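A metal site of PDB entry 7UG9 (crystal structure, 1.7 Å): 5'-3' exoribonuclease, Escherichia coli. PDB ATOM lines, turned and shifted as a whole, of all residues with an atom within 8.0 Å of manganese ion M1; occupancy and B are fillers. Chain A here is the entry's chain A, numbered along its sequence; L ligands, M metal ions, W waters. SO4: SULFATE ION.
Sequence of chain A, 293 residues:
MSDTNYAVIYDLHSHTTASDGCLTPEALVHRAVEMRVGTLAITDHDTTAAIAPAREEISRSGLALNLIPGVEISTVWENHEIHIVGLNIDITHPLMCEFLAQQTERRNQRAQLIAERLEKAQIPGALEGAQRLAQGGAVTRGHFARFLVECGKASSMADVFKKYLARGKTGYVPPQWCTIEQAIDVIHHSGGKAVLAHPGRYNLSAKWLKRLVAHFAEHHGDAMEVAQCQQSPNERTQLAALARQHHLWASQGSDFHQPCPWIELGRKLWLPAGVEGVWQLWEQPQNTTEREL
OD1 of Asp 20 sits at hydrogen-bond distance from ND1 of His 15 (3.3 Å). OD1 of Asp 20 sits at hydrogen-bond distance from OG of Ser 19. A ring nitrogen (ND1) of His 257 lies within hydrogen-bond range of the backbone carbonyl oxygen of Asp 255, at 2.9 Å. The side-chain hydroxyl of Ser 19 is in hydrogen-bond range of the backbone NH of His 45 (3.3 Å). The side-chain hydroxyl of Ser 19 sits at hydrogen-bond distance from a ring nitrogen (ND1) of His 15. N of His 15 is in hydrogen-bond range of O of Phe 256 (2.9 Å).
His 15 touches manganese ion M1 (CE1 to MN, 3.7 Å). Four residues have an atom within 4 Å of manganese ion M1: His 15, Asp 20, His 45 and His 257. The nearest printed residue that does not touch manganese ion M1 is Asp 255 (5.0 Å).
Manganese ion M1 is bound by water W1, O3 of the ligand, OD2 of Asp 20, NE2 of His 257 and NE2 of His 45. Slightly farther from manganese ion M1 lies the side-chain carboxylate (OD1) of Asp 20 (2.7 Å).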
ATOM      1  N   HIS A  13     -12.889  31.943  14.832  1.00  0.00           N
ATOM      2  CA  HIS A  13     -11.840  31.086  14.291  1.00  0.00           C
ATOM      3  C   HIS A  13     -11.904  31.190  12.767  1.00  0.00           C
ATOM      4  O   HIS A  13     -12.835  30.658  12.168  1.00  0.00           O
ATOM      5  CB  HIS A  13     -12.014  29.647  14.757  1.00  0.00           C
ATOM      6  CG  HIS A  13     -10.807  28.773  14.519  1.00  0.00           C
ATOM      7  ND1 HIS A  13     -10.407  27.811  15.418  1.00  0.00           N
ATOM      8  CD2 HIS A  13      -9.936  28.712  13.482  1.00  0.00           C
ATOM      9  CE1 HIS A  13      -9.348  27.179  14.936  1.00  0.00           C
ATOM     10  NE2 HIS A  13      -9.029  27.705  13.769  1.00  0.00           N
ATOM     11  N   SER A  14     -10.931  31.871  12.169  1.00  0.00           N
ATOM     12  CA  SER A  14     -10.922  32.039  10.711  1.00  0.00           C
ATOM     13  C   SER A  14      -9.498  32.285  10.243  1.00  0.00           C
ATOM     14  O   SER A  14      -8.627  32.705  11.028  1.00  0.00           O
ATOM     15  CB  SER A  14     -11.812  33.216  10.279  1.00  0.00           C
ATOM     16  OG  SER A  14     -11.296  34.438  10.791  1.00  0.00           O
ATOM     17  N   HIS A  15      -9.263  32.031   8.957  1.00  0.00           N
ATOM     18  CA  HIS A  15      -7.927  32.146   8.370  1.00  0.00           C
ATOM     19  C   HIS A  15      -7.941  33.022   7.125  1.00  0.00           C
ATOM     20  O   HIS A  15      -8.971  33.179   6.467  1.00  0.00           O
ATOM     21  CB  HIS A  15      -7.356  30.778   7.997  1.00  0.00           C
ATOM     22  CG  HIS A  15      -7.126  29.914   9.187  1.00  0.00           C
ATOM     23  ND1 HIS A  15      -5.882  29.764   9.742  1.00  0.00           N
ATOM     24  CD2 HIS A  15      -7.964  29.140   9.905  1.00  0.00           C
ATOM     25  CE1 HIS A  15      -5.969  28.957  10.791  1.00  0.00           C
ATOM     26  NE2 HIS A  15      -7.217  28.566  10.912  1.00  0.00           N
ATOM     27  N   THR A  16      -6.786  33.619   6.851  1.00  0.00           N
ATOM     28  CA  THR A  16      -6.569  34.491   5.696  1.00  0.00           C
ATOM     29  C   THR A  16      -5.324  34.029   4.966  1.00  0.00           C
ATOM     30  O   THR A  16      -4.620  33.114   5.412  1.00  0.00           O
ATOM     31  CB  THR A  16      -6.332  35.942   6.114  1.00  0.00           C
ATOM     32  OG1 THR A  16      -5.056  36.031   6.778  1.00  0.00           O
ATOM     33  CG2 THR A  16      -7.442  36.420   7.040  1.00  0.00           C
ATOM     34  N   SER A  19      -1.968  33.046   6.647  1.00  0.00           N
ATOM     35  CA  SER A  19      -1.567  31.657   6.868  1.00  0.00           C
ATOM     36  C   SER A  19      -2.089  30.813   5.722  1.00  0.00           C
ATOM     37  O   SER A  19      -1.668  30.993   4.575  1.00  0.00           O
ATOM     38  CB  SER A  19      -2.006  31.141   8.253  1.00  0.00           C
ATOM     39  OG  SER A  19      -3.393  31.010   8.444  1.00  0.00           O
ATOM     40  N   ASP A  20      -3.036  29.910   5.973  1.00  0.00           N
ATOM     41  CA  ASP A  20      -3.432  28.986   4.909  1.00  0.00           C
ATOM     42  C   ASP A  20      -4.852  29.237   4.401  1.00  0.00           C
ATOM     43  O   ASP A  20      -5.447  28.333   3.819  1.00  0.00           O
ATOM     44  CB  ASP A  20      -3.263  27.532   5.354  1.00  0.00           C
ATOM     45  CG  ASP A  20      -4.057  27.182   6.603  1.00  0.00           C
ATOM     46  OD1 ASP A  20      -4.595  28.106   7.249  1.00  0.00           O
ATOM     47  OD2 ASP A  20      -4.143  25.986   6.937  1.00  0.00           O
ATOM     48  N   GLY A  21      -5.382  30.448   4.601  1.00  0.00           N
ATOM     49  CA  GLY A  21      -6.634  30.804   3.987  1.00  0.00           C
ATOM     50  C   GLY A  21      -6.429  31.300   2.565  1.00  0.00           C
ATOM     51  O   GLY A  21      -5.324  31.656   2.168  1.00  0.00           O
ATOM     52  N   THR A  43      -7.648  34.134  13.223  1.00  0.00           N
ATOM     53  CA  THR A  43      -6.815  33.254  14.042  1.00  0.00           C
ATOM     54  C   THR A  43      -5.868  32.472  13.114  1.00  0.00           C
ATOM     55  O   THR A  43      -5.924  31.250  13.024  1.00  0.00           O
ATOM     56  CB  THR A  43      -7.678  32.320  14.899  1.00  0.00           C
ATOM     57  OG1 THR A  43      -8.495  31.459  14.083  1.00  0.00           O
ATOM     58  CG2 THR A  43      -8.595  33.129  15.852  1.00  0.00           C
ATOM     59  N   ASP A  44      -4.990  33.195  12.423  1.00  0.00           N
ATOM     60  CA  ASP A  44      -4.052  32.572  11.496  1.00  0.00           C
ATOM     61  C   ASP A  44      -3.019  31.733  12.260  1.00  0.00           C
ATOM     62  O   ASP A  44      -2.723  31.995  13.416  1.00  0.00           O
ATOM     63  CB  ASP A  44      -3.382  33.651  10.646  1.00  0.00           C
ATOM     64  CG  ASP A  44      -4.216  34.051   9.422  1.00  0.00           C
ATOM     65  OD1 ASP A  44      -4.744  33.151   8.731  1.00  0.00           O
ATOM     66  OD2 ASP A  44      -4.445  35.264   9.221  1.00  0.00           O
ATOM     67  N   HIS A  45      -2.497  30.695  11.589  1.00  0.00           N
ATOM     68  CA  HIS A  45      -1.477  29.835  12.187  1.00  0.00           C
ATOM     69  C   HIS A  45      -0.209  30.593  12.508  1.00  0.00           C
ATOM     70  O   HIS A  45       0.498  31.058  11.603  1.00  0.00           O
ATOM     71  CB  HIS A  45      -1.149  28.669  11.247  1.00  0.00           C
ATOM     72  CG  HIS A  45      -2.296  27.750  10.995  1.00  0.00           C
ATOM     73  ND1 HIS A  45      -2.775  26.888  11.951  1.00  0.00           N
ATOM     74  CD2 HIS A  45      -3.051  27.555   9.892  1.00  0.00           C
ATOM     75  CE1 HIS A  45      -3.780  26.192  11.448  1.00  0.00           C
ATOM     76  NE2 HIS A  45      -3.989  26.596  10.207  1.00  0.00           N
ATOM     77  N   GLU A  72      -3.727  31.204  15.999  1.00  0.00           N
ATOM     78  CA  GLU A  72      -3.832  29.771  16.264  1.00  0.00           C
ATOM     79  C   GLU A  72      -2.436  29.203  16.432  1.00  0.00           C
ATOM     80  O   GLU A  72      -1.629  29.256  15.503  1.00  0.00           O
ATOM     81  CB  GLU A  72      -4.584  29.047  15.150  1.00  0.00           C
ATOM     82  CG  GLU A  72      -4.925  27.603  15.616  1.00  0.00           C
ATOM     83  CD  GLU A  72      -5.764  26.829  14.647  1.00  0.00           C
ATOM     84  OE1 GLU A  72      -5.973  27.326  13.524  1.00  0.00           O
ATOM     85  OE2 GLU A  72      -6.290  25.761  15.047  1.00  0.00           O
ATOM     86  N   HIS A  83      -4.139  22.266  18.825  1.00  0.00           N
ATOM     87  CA  HIS A  83      -4.168  23.665  18.438  1.00  0.00           C
ATOM     88  C   HIS A  83      -4.836  24.492  19.533  1.00  0.00           C
ATOM     89  O   HIS A  83      -5.932  24.153  19.984  1.00  0.00           O
ATOM     90  CB  HIS A  83      -4.900  23.857  17.093  1.00  0.00           C
ATOM     91  CG  HIS A  83      -4.167  23.264  15.921  1.00  0.00           C
ATOM     92  ND1 HIS A  83      -4.741  23.089  14.679  1.00  0.00           N
ATOM     93  CD2 HIS A  83      -2.903  22.770  15.817  1.00  0.00           C
ATOM     94  CE1 HIS A  83      -3.860  22.541  13.849  1.00  0.00           C
ATOM     95  NE2 HIS A  83      -2.733  22.351  14.521  1.00  0.00           N
ATOM     96  N   HIS A 198     -11.180  23.163  18.177  1.00  0.00           N
ATOM     97  CA  HIS A 198     -11.836  22.029  17.525  1.00  0.00           C
ATOM     98  C   HIS A 198     -11.531  20.715  18.234  1.00  0.00           C
ATOM     99  O   HIS A 198     -10.851  19.838  17.686  1.00  0.00           O
ATOM    100  CB  HIS A 198     -11.467  21.952  16.028  1.00  0.00           C
ATOM    101  CG  HIS A 198     -10.026  22.241  15.706  1.00  0.00           C
ATOM    102  ND1 HIS A 198      -8.990  21.420  16.078  1.00  0.00           N
ATOM    103  CD2 HIS A 198      -9.472  23.250  14.989  1.00  0.00           C
ATOM    104  CE1 HIS A 198      -7.850  21.922  15.647  1.00  0.00           C
ATOM    105  NE2 HIS A 198      -8.110  23.033  14.969  1.00  0.00           N
ATOM    106  N   ARG A 201     -11.927  17.212  16.516  1.00  0.00           N
ATOM    107  CA  ARG A 201     -11.061  16.819  15.397  1.00  0.00           C
ATOM    108  C   ARG A 201      -9.865  16.004  15.817  1.00  0.00           C
ATOM    109  O   ARG A 201      -9.194  15.422  14.958  1.00  0.00           O
ATOM    110  CB  ARG A 201     -10.573  18.052  14.629  1.00  0.00           C
ATOM    111  CG  ARG A 201     -11.491  18.426  13.498  1.00  0.00           C
ATOM    112  CD  ARG A 201     -10.887  19.433  12.520  1.00  0.00           C
ATOM    113  NE  ARG A 201      -9.434  19.543  12.540  1.00  0.00           N
ATOM    114  CZ  ARG A 201      -8.791  20.597  12.070  1.00  0.00           C
ATOM    115  NH1 ARG A 201      -9.437  21.622  11.560  1.00  0.00           N
ATOM    116  NH2 ARG A 201      -7.453  20.639  12.133  1.00  0.00           N
ATOM    117  N   ASP A 255     -13.653  28.027  11.526  1.00  0.00           N
ATOM    118  CA  ASP A 255     -12.378  27.588  10.978  1.00  0.00           C
ATOM    119  C   ASP A 255     -12.354  27.782   9.472  1.00  0.00           C
ATOM    120  O   ASP A 255     -11.840  26.958   8.722  1.00  0.00           O
ATOM    121  CB  ASP A 255     -12.106  26.125  11.326  1.00  0.00           C
ATOM    122  CG  ASP A 255     -10.652  25.774  11.304  1.00  0.00           C
ATOM    123  OD1 ASP A 255      -9.808  26.658  11.076  1.00  0.00           O
ATOM    124  OD2 ASP A 255     -10.346  24.574  11.472  1.00  0.00           O
ATOM    125  N   PHE A 256     -12.955  28.879   9.034  1.00  0.00           N
ATOM    126  CA  PHE A 256     -13.025  29.176   7.604  1.00  0.00           C
ATOM    127  C   PHE A 256     -11.639  29.335   6.991  1.00  0.00           C
ATOM    128  O   PHE A 256     -10.820  30.108   7.475  1.00  0.00           O
ATOM    129  CB  PHE A 256     -13.836  30.454   7.413  1.00  0.00           C
ATOM    130  CG  PHE A 256     -13.931  30.900   5.989  1.00  0.00           C
ATOM    131  CD1 PHE A 256     -12.961  31.715   5.430  1.00  0.00           C
ATOM    132  CD2 PHE A 256     -15.002  30.494   5.212  1.00  0.00           C
ATOM    133  CE1 PHE A 256     -13.066  32.133   4.096  1.00  0.00           C
ATOM    134  CE2 PHE A 256     -15.126  30.924   3.912  1.00  0.00           C
ATOM    135  CZ  PHE A 256     -14.136  31.725   3.352  1.00  0.00           C
ATOM    136  N   HIS A 257     -11.418  28.633   5.876  1.00  0.00           N
ATOM    137  CA  HIS A 257     -10.230  28.819   5.036  1.00  0.00           C
ATOM    138  C   HIS A 257     -10.575  29.339   3.646  1.00  0.00           C
ATOM    139  O   HIS A 257      -9.912  30.238   3.148  1.00  0.00           O
ATOM    140  CB  HIS A 257      -9.465  27.500   4.871  1.00  0.00           C
ATOM    141  CG  HIS A 257      -8.725  27.071   6.089  1.00  0.00           C
ATOM    142  ND1 HIS A 257      -9.364  26.665   7.242  1.00  0.00           N
ATOM    143  CD2 HIS A 257      -7.391  26.923   6.332  1.00  0.00           C
ATOM    144  CE1 HIS A 257      -8.472  26.315   8.143  1.00  0.00           C
ATOM    145  NE2 HIS A 257      -7.263  26.484   7.628  1.00  0.00           N
HETATM  146  S   SO4 L   1      -6.989  24.282  11.223  1.00  0.00           S
HETATM  147  O1  SO4 L   1      -5.925  23.432  11.756  1.00  0.00           O
HETATM  148  O2  SO4 L   1      -7.628  24.866  12.404  1.00  0.00           O
HETATM  149  O3  SO4 L   1      -6.530  25.378  10.387  1.00  0.00           O
HETATM  150  O4  SO4 L   1      -7.942  23.479  10.460  1.00  0.00           O
HETATM  151 MN    MN M   1      -5.445  25.915   8.673  1.00  0.00          MN
HETATM  152 MN    MN M   2      -7.747  26.944  12.200  1.00  0.00          MN
HETATM  153 MN    MN M   3      -6.517  24.028  14.009  1.00  0.00          MN
HETATM  154  O   HOH W   1      -5.050  23.897   8.566  1.00  0.00           O
